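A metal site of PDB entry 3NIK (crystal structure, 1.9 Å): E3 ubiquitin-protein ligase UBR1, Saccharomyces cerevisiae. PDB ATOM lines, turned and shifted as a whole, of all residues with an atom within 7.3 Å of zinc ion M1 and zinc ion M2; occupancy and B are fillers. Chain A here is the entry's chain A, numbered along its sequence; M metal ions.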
ATOM      1  N   HIS A   4      17.899  18.703 -21.679  1.00  0.00           N
ATOM      2  CA  HIS A   4      16.457  18.672 -21.699  1.00  0.00           C
ATOM      3  C   HIS A   4      15.906  17.557 -20.794  1.00  0.00           C
ATOM      4  O   HIS A   4      16.362  16.420 -20.853  1.00  0.00           O
ATOM      5  CB  HIS A   4      15.973  18.483 -23.131  1.00  0.00           C
ATOM      6  CG  HIS A   4      14.560  18.923 -23.348  1.00  0.00           C
ATOM      7  ND1 HIS A   4      13.488  18.055 -23.214  1.00  0.00           N
ATOM      8  CD2 HIS A   4      14.035  20.123 -23.664  1.00  0.00           C
ATOM      9  CE1 HIS A   4      12.373  18.715 -23.458  1.00  0.00           C
ATOM     10  NE2 HIS A   4      12.672  19.973 -23.734  1.00  0.00           N
ATOM     11  N   LYS A   5      14.938  17.903 -19.934  1.00  0.00           N
ATOM     12  CA  LYS A   5      14.191  16.886 -19.174  1.00  0.00           C
ATOM     13  C   LYS A   5      13.061  16.377 -20.050  1.00  0.00           C
ATOM     14  O   LYS A   5      12.466  17.144 -20.804  1.00  0.00           O
ATOM     15  CB  LYS A   5      13.541  17.468 -17.906  1.00  0.00           C
ATOM     16  CG  LYS A   5      14.483  17.955 -16.830  1.00  0.00           C
ATOM     17  CD  LYS A   5      13.704  18.724 -15.774  1.00  0.00           C
ATOM     18  CE  LYS A   5      14.584  19.686 -14.980  1.00  0.00           C
ATOM     19  NZ  LYS A   5      15.491  19.010 -14.018  1.00  0.00           N
ATOM     20  N   HIS A   6      12.735  15.094 -19.921  1.00  0.00           N
ATOM     21  CA  HIS A   6      11.585  14.543 -20.624  1.00  0.00           C
ATOM     22  C   HIS A   6      10.553  14.019 -19.627  1.00  0.00           C
ATOM     23  O   HIS A   6       9.982  12.945 -19.809  1.00  0.00           O
ATOM     24  CB  HIS A   6      12.046  13.442 -21.594  1.00  0.00           C
ATOM     25  CG  HIS A   6      12.783  12.320 -20.931  1.00  0.00           C
ATOM     26  ND1 HIS A   6      12.135  11.204 -20.424  1.00  0.00           N
ATOM     27  CD2 HIS A   6      14.100  12.126 -20.693  1.00  0.00           C
ATOM     28  CE1 HIS A   6      13.032  10.383 -19.899  1.00  0.00           C
ATOM     29  NE2 HIS A   6      14.221  10.926 -20.046  1.00  0.00           N
ATOM     30  N   ARG A   9       7.304  11.292 -19.857  1.00  0.00           N
ATOM     31  CA  ARG A   9       7.382  10.517 -21.091  1.00  0.00           C
ATOM     32  C   ARG A   9       8.766   9.875 -21.227  1.00  0.00           C
ATOM     33  O   ARG A   9       9.627  10.049 -20.369  1.00  0.00           O
ATOM     34  CB  ARG A   9       7.082  11.393 -22.321  1.00  0.00           C
ATOM     35  CG  ARG A   9       7.959  12.637 -22.444  1.00  0.00           C
ATOM     36  CD  ARG A   9       8.020  13.173 -23.884  1.00  0.00           C
ATOM     37  NE  ARG A   9       8.981  12.441 -24.721  1.00  0.00           N
ATOM     38  CZ  ARG A   9       9.386  12.815 -25.932  1.00  0.00           C
ATOM     39  NH1 ARG A   9       8.932  13.941 -26.502  1.00  0.00           N
ATOM     40  NH2 ARG A   9      10.271  12.066 -26.591  1.00  0.00           N
ATOM     41  N   ASN A  10       8.947   9.122 -22.300  1.00  0.00           N
ATOM     42  CA  ASN A  10      10.232   8.498 -22.622  1.00  0.00           C
ATOM     43  C   ASN A  10      11.171   9.544 -23.207  1.00  0.00           C
ATOM     44  O   ASN A  10      10.726  10.602 -23.665  1.00  0.00           O
ATOM     45  CB  ASN A  10      10.040   7.390 -23.652  1.00  0.00           C
ATOM     46  CG  ASN A  10       9.583   7.946 -24.981  1.00  0.00           C
ATOM     47  OD1 ASN A  10       8.591   8.674 -25.052  1.00  0.00           O
ATOM     48  ND2 ASN A  10      10.333   7.658 -26.048  1.00  0.00           N
ATOM     49  N   CYS A  11      12.477   9.256 -23.198  1.00  0.00           N
ATOM     50  CA  CYS A  11      13.461  10.140 -23.818  1.00  0.00           C
ATOM     51  C   CYS A  11      13.338  10.046 -25.340  1.00  0.00           C
ATOM     52  O   CYS A  11      12.920  11.011 -26.012  1.00  0.00           O
ATOM     53  CB  CYS A  11      14.881   9.769 -23.358  1.00  0.00           C
ATOM     54  SG  CYS A  11      16.178  10.681 -24.203  1.00  0.00           S
ATOM     55  N   GLY A  12      13.683   8.886 -25.886  1.00  0.00           N
ATOM     56  CA  GLY A  12      13.551   8.618 -27.322  1.00  0.00           C
ATOM     57  C   GLY A  12      14.554   9.347 -28.189  1.00  0.00           C
ATOM     58  O   GLY A  12      14.395   9.416 -29.412  1.00  0.00           O
ATOM     59  N   ARG A  13      15.585   9.905 -27.565  1.00  0.00           N
ATOM     60  CA  ARG A  13      16.628  10.624 -28.285  1.00  0.00           C
ATOM     61  C   ARG A  13      17.387   9.723 -29.251  1.00  0.00           C
ATOM     62  O   ARG A  13      17.932   8.701 -28.840  1.00  0.00           O
ATOM     63  CB  ARG A  13      17.628  11.248 -27.296  1.00  0.00           C
ATOM     64  CG  ARG A  13      18.569  12.258 -27.902  1.00  0.00           C
ATOM     65  CD  ARG A  13      19.383  12.924 -26.783  1.00  0.00           C
ATOM     66  NE  ARG A  13      20.535  13.633 -27.308  1.00  0.00           N
ATOM     67  CZ  ARG A  13      21.693  13.062 -27.653  1.00  0.00           C
ATOM     68  NH1 ARG A  13      21.865  11.748 -27.528  1.00  0.00           N
ATOM     69  NH2 ARG A  13      22.670  13.815 -28.125  1.00  0.00           N
ATOM     70  N   PHE A  15      20.573   8.667 -31.105  1.00  0.00           N
ATOM     71  CA  PHE A  15      21.985   8.839 -30.787  1.00  0.00           C
ATOM     72  C   PHE A  15      22.697   9.564 -31.913  1.00  0.00           C
ATOM     73  O   PHE A  15      22.312   9.428 -33.081  1.00  0.00           O
ATOM     74  CB  PHE A  15      22.680   7.503 -30.500  1.00  0.00           C
ATOM     75  CG  PHE A  15      22.183   6.826 -29.267  1.00  0.00           C
ATOM     76  CD1 PHE A  15      22.783   7.054 -28.030  1.00  0.00           C
ATOM     77  CD2 PHE A  15      21.088   5.970 -29.330  1.00  0.00           C
ATOM     78  CE1 PHE A  15      22.312   6.445 -26.885  1.00  0.00           C
ATOM     79  CE2 PHE A  15      20.596   5.350 -28.177  1.00  0.00           C
ATOM     80  CZ  PHE A  15      21.208   5.592 -26.954  1.00  0.00           C
ATOM     81  N   VAL A  34      18.803   0.634 -24.062  1.00  0.00           N
ATOM     82  CA  VAL A  34      19.951   1.547 -23.998  1.00  0.00           C
ATOM     83  C   VAL A  34      19.574   2.916 -23.435  1.00  0.00           C
ATOM     84  O   VAL A  34      18.407   3.332 -23.491  1.00  0.00           O
ATOM     85  CB  VAL A  34      20.624   1.746 -25.379  1.00  0.00           C
ATOM     86  CG1 VAL A  34      21.311   0.458 -25.836  1.00  0.00           C
ATOM     87  CG2 VAL A  34      19.623   2.231 -26.439  1.00  0.00           C
ATOM     88  N   LEU A  35      20.575   3.609 -22.896  1.00  0.00           N
ATOM     89  CA  LEU A  35      20.426   4.937 -22.312  1.00  0.00           C
ATOM     90  C   LEU A  35      21.431   5.886 -22.914  1.00  0.00           C
ATOM     91  O   LEU A  35      22.572   5.498 -23.200  1.00  0.00           O
ATOM     92  CB  LEU A  35      20.625   4.884 -20.787  1.00  0.00           C
ATOM     93  CG  LEU A  35      19.592   4.071 -20.010  1.00  0.00           C
ATOM     94  CD1 LEU A  35      20.048   3.795 -18.564  1.00  0.00           C
ATOM     95  CD2 LEU A  35      18.231   4.772 -20.004  1.00  0.00           C
ATOM     96  N   CYS A  36      20.990   7.117 -23.154  1.00  0.00           N
ATOM     97  CA  CYS A  36      21.864   8.150 -23.676  1.00  0.00           C
ATOM     98  C   CYS A  36      22.598   8.867 -22.561  1.00  0.00           C
ATOM     99  O   CYS A  36      22.330   8.657 -21.378  1.00  0.00           O
ATOM    100  CB  CYS A  36      21.075   9.168 -24.524  1.00  0.00           C
ATOM    101  SG  CYS A  36      20.130  10.374 -23.558  1.00  0.00           S
ATOM    102  N   ILE A  37      23.501   9.745 -22.967  1.00  0.00           N
ATOM    103  CA  ILE A  37      24.381  10.453 -22.038  1.00  0.00           C
ATOM    104  C   ILE A  37      23.641  11.488 -21.198  1.00  0.00           C
ATOM    105  O   ILE A  37      24.073  11.803 -20.078  1.00  0.00           O
ATOM    106  CB  ILE A  37      25.579  11.085 -22.798  1.00  0.00           C
ATOM    107  CG1 ILE A  37      25.129  12.255 -23.674  1.00  0.00           C
ATOM    108  CG2 ILE A  37      26.276  10.031 -23.597  1.00  0.00           C
ATOM    109  CD1 ILE A  37      26.027  12.521 -24.875  1.00  0.00           C
ATOM    110  N   HIS A  38      22.525  11.992 -21.716  1.00  0.00           N
ATOM    111  CA  HIS A  38      21.675  12.919 -20.965  1.00  0.00           C
ATOM    112  C   HIS A  38      21.058  12.204 -19.772  1.00  0.00           C
ATOM    113  O   HIS A  38      20.821  12.817 -18.735  1.00  0.00           O
ATOM    114  CB  HIS A  38      20.526  13.472 -21.825  1.00  0.00           C
ATOM    115  CG  HIS A  38      20.958  14.268 -23.012  1.00  0.00           C
ATOM    116  ND1 HIS A  38      22.250  14.284 -23.491  1.00  0.00           N
ATOM    117  CD2 HIS A  38      20.251  15.062 -23.847  1.00  0.00           C
ATOM    118  CE1 HIS A  38      22.318  15.069 -24.557  1.00  0.00           C
ATOM    119  NE2 HIS A  38      21.121  15.555 -24.789  1.00  0.00           N
ATOM    120  N   CYS A  39      20.812  10.898 -19.928  1.00  0.00           N
ATOM    121  CA  CYS A  39      19.931  10.148 -19.033  1.00  0.00           C
ATOM    122  C   CYS A  39      20.634   9.206 -18.065  1.00  0.00           C
ATOM    123  O   CYS A  39      20.215   9.065 -16.917  1.00  0.00           O
ATOM    124  CB  CYS A  39      18.948   9.331 -19.885  1.00  0.00           C
ATOM    125  SG  CYS A  39      17.722  10.378 -20.713  1.00  0.00           S
ATOM    126  N   PHE A  40      21.655   8.523 -18.579  1.00  0.00           N
ATOM    127  CA  PHE A  40      22.344   7.480 -17.817  1.00  0.00           C
ATOM    128  C   PHE A  40      22.849   8.055 -16.510  1.00  0.00           C
ATOM    129  O   PHE A  40      23.619   9.010 -16.518  1.00  0.00           O
ATOM    130  CB  PHE A  40      23.512   6.930 -18.630  1.00  0.00           C
ATOM    131  CG  PHE A  40      24.352   5.918 -17.883  1.00  0.00           C
ATOM    132  CD1 PHE A  40      23.932   4.599 -17.777  1.00  0.00           C
ATOM    133  CD2 PHE A  40      25.554   6.293 -17.274  1.00  0.00           C
ATOM    134  CE1 PHE A  40      24.701   3.658 -17.096  1.00  0.00           C
ATOM    135  CE2 PHE A  40      26.340   5.356 -16.581  1.00  0.00           C
ATOM    136  CZ  PHE A  40      25.919   4.052 -16.485  1.00  0.00           C
ATOM    137  N   ILE A  62      17.546   4.703 -30.333  1.00  0.00           N
ATOM    138  CA  ILE A  62      16.967   5.772 -29.524  1.00  0.00           C
ATOM    139  C   ILE A  62      17.020   5.394 -28.055  1.00  0.00           C
ATOM    140  O   ILE A  62      16.947   4.209 -27.719  1.00  0.00           O
ATOM    141  CB  ILE A  62      15.500   6.121 -29.935  1.00  0.00           C
ATOM    142  CG1 ILE A  62      14.622   4.867 -29.975  1.00  0.00           C
ATOM    143  CG2 ILE A  62      15.479   6.839 -31.287  1.00  0.00           C
ATOM    144  CD1 ILE A  62      13.768   4.684 -28.786  1.00  0.00           C
ATOM    145  N   CYS A  63      17.145   6.407 -27.203  1.00  0.00           N
ATOM    146  CA  CYS A  63      17.261   6.213 -25.769  1.00  0.00           C
ATOM    147  C   CYS A  63      15.947   5.691 -25.184  1.00  0.00           C
ATOM    148  O   CYS A  63      14.878   6.199 -25.497  1.00  0.00           O
ATOM    149  CB  CYS A  63      17.676   7.516 -25.094  1.00  0.00           C
ATOM    150  SG  CYS A  63      17.712   7.412 -23.323  1.00  0.00           S
ATOM    151  N   ASP A  64      16.043   4.679 -24.322  1.00  0.00           N
ATOM    152  CA  ASP A  64      14.874   4.044 -23.692  1.00  0.00           C
ATOM    153  C   ASP A  64      14.548   4.562 -22.294  1.00  0.00           C
ATOM    154  O   ASP A  64      13.635   4.061 -21.643  1.00  0.00           O
ATOM    155  CB  ASP A  64      15.042   2.504 -23.651  1.00  0.00           C
ATOM    156  CG  ASP A  64      15.160   1.906 -25.024  1.00  0.00           C
ATOM    157  OD1 ASP A  64      14.227   2.050 -25.864  1.00  0.00           O
ATOM    158  OD2 ASP A  64      16.212   1.275 -25.282  1.00  0.00           O
ATOM    159  N   CYS A  65      15.285   5.567 -21.820  1.00  0.00           N
ATOM    160  CA  CYS A  65      14.954   6.158 -20.518  1.00  0.00           C
ATOM    161  C   CYS A  65      13.485   6.593 -20.503  1.00  0.00           C
ATOM    162  O   CYS A  65      13.025   7.258 -21.412  1.00  0.00           O
ATOM    163  CB  CYS A  65      15.853   7.371 -20.253  1.00  0.00           C
ATOM    164  SG  CYS A  65      15.655   8.038 -18.572  1.00  0.00           S
ATOM    165  N   GLY A  66      12.749   6.206 -19.470  1.00  0.00           N
ATOM    166  CA  GLY A  66      11.334   6.620 -19.374  1.00  0.00           C
ATOM    167  C   GLY A  66      10.342   5.720 -20.093  1.00  0.00           C
ATOM    168  O   GLY A  66       9.131   5.965 -20.061  1.00  0.00           O
ATOM    169  N   LEU A  75      14.567   3.794 -12.892  1.00  0.00           N
ATOM    170  CA  LEU A  75      15.698   4.652 -13.247  1.00  0.00           C
ATOM    171  C   LEU A  75      15.507   6.069 -12.730  1.00  0.00           C
ATOM    172  O   LEU A  75      14.386   6.556 -12.628  1.00  0.00           O
ATOM    173  CB  LEU A  75      15.906   4.713 -14.766  1.00  0.00           C
ATOM    174  CG  LEU A  75      16.186   3.423 -15.548  1.00  0.00           C
ATOM    175  CD1 LEU A  75      16.320   3.739 -17.017  1.00  0.00           C
ATOM    176  CD2 LEU A  75      17.435   2.712 -15.053  1.00  0.00           C
ATOM    177  N   HIS A  76      16.617   6.725 -12.411  1.00  0.00           N
ATOM    178  CA  HIS A  76      16.591   8.105 -11.965  1.00  0.00           C
ATOM    179  C   HIS A  76      17.316   8.943 -13.017  1.00  0.00           C
ATOM    180  O   HIS A  76      18.522   9.185 -12.920  1.00  0.00           O
ATOM    181  CB  HIS A  76      17.200   8.222 -10.577  1.00  0.00           C
ATOM    182  CG  HIS A  76      16.517   7.370  -9.562  1.00  0.00           C
ATOM    183  ND1 HIS A  76      16.875   6.063  -9.322  1.00  0.00           N
ATOM    184  CD2 HIS A  76      15.453   7.615  -8.753  1.00  0.00           C
ATOM    185  CE1 HIS A  76      16.081   5.547  -8.396  1.00  0.00           C
ATOM    186  NE2 HIS A  76      15.209   6.472  -8.030  1.00  0.00           N
ATOM    187  N   CYS A  77      16.571   9.366 -14.032  1.00  0.00           N
ATOM    188  CA  CYS A  77      17.128  10.079 -15.167  1.00  0.00           C
ATOM    189  C   CYS A  77      18.037  11.200 -14.683  1.00  0.00           C
ATOM    190  O   CYS A  77      17.601  12.057 -13.916  1.00  0.00           O
ATOM    191  CB  CYS A  77      15.998  10.679 -16.015  1.00  0.00           C
ATOM    192  SG  CYS A  77      16.562  11.655 -17.412  1.00  0.00           S
ATOM    193  N   LYS A  78      19.286  11.175 -15.151  1.00  0.00           N
ATOM    194  CA  LYS A  78      20.290  12.195 -14.814  1.00  0.00           C
ATOM    195  C   LYS A  78      19.825  13.618 -15.121  1.00  0.00           C
ATOM    196  O   LYS A  78      20.144  14.557 -14.366  1.00  0.00           O
ATOM    197  CB  LYS A  78      21.632  11.905 -15.507  1.00  0.00           C
ATOM    198  CG  LYS A  78      22.802  12.666 -14.875  1.00  0.00           C
ATOM    199  CD  LYS A  78      24.125  12.439 -15.565  1.00  0.00           C
ATOM    200  CE  LYS A  78      25.224  13.251 -14.869  1.00  0.00           C
ATOM    201  NZ  LYS A  78      26.588  12.872 -15.323  1.00  0.00           N
ATOM    202  N   ALA A  79      19.090  13.791 -16.215  1.00  0.00           N
ATOM    203  CA  ALA A  79      18.574  15.119 -16.604  1.00  0.00           C
ATOM    204  C   ALA A  79      17.711  15.750 -15.517  1.00  0.00           C
ATOM    205  O   ALA A  79      17.638  16.979 -15.410  1.00  0.00           O
ATOM    206  CB  ALA A  79      17.807  15.042 -17.929  1.00  0.00           C
ATOM    207  N   GLU A  80      17.050  14.925 -14.725  1.00  0.00           N
ATOM    208  CA  GLU A  80      16.174  15.410 -13.670  1.00  0.00           C
ATOM    209  C   GLU A  80      16.937  15.982 -12.473  1.00  0.00           C
ATOM    210  O   GLU A  80      16.365  16.674 -11.641  1.00  0.00           O
ATOM    211  CB  GLU A  80      15.235  14.295 -13.200  1.00  0.00           C
ATOM    212  CG  GLU A  80      14.268  13.759 -14.279  1.00  0.00           C
ATOM    213  CD  GLU A  80      13.086  14.685 -14.540  1.00  0.00           C
ATOM    214  OE1 GLU A  80      12.795  15.561 -13.683  1.00  0.00           O
ATOM    215  OE2 GLU A  80      12.456  14.542 -15.604  1.00  0.00           O
HETATM  216 ZN    ZN M   1      17.970   9.664 -23.061  1.00  0.00          ZN
HETATM  217 ZN    ZN M   2      16.044  10.253 -19.166  1.00  0.00          ZN
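The side-chain sulfur (SG) of Cys 63 is bound to zinc ion M1, 2.3 Å away. Zinc ion M1 is bound by SG of Cys 36, 2.3 Å away. Zinc ion M1 is bound by SG of Cys 11 (2.4 Å). Zinc ion M1 is bound by the side-chain sulfur (SG) of Cys 39 (2.5 Å).
ND1 of His 6 sits at hydrogen-bond distance from O of Arg 9, 2.8 Å away. The backbone NH of Cys 65 lies close to the side-chain sulfur of Cys 63 (3.4 Å). N of Cys 63 is in hydrogen-bond range of O of Arg 13, 2.9 Å away. The backbone NH of Gly 12 sits at hydrogen-bond distance from the backbone carbonyl oxygen of Cys 63 (3.0 Å). O of Cys 39 is in hydrogen-bond range of N of Lys 78 (2.9 Å). SG of Cys 77 sits close to N of Ala 79. N of Cys 11 is in hydrogen-bond range of O of Cys 65 (2.7 Å). O of Cys 11 sits at hydrogen-bond distance from NH2 of Arg 9 (2.9 Å).
Of the 27 residues printed, 4 come within 4 Å of zinc ion M2. The nearest printed residue that does not touch zinc ion M2 is Cys 11 (4.4 Å).
Zinc ion M2 is bound by NE2 of His 6 (2.1 Å), SG of Cys 39 (2.3 Å), SG of Cys 77 (2.3 Å) and SG of Cys 65 (2.3 Å). Zinc ion M2 has four donor atoms within binding distance.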
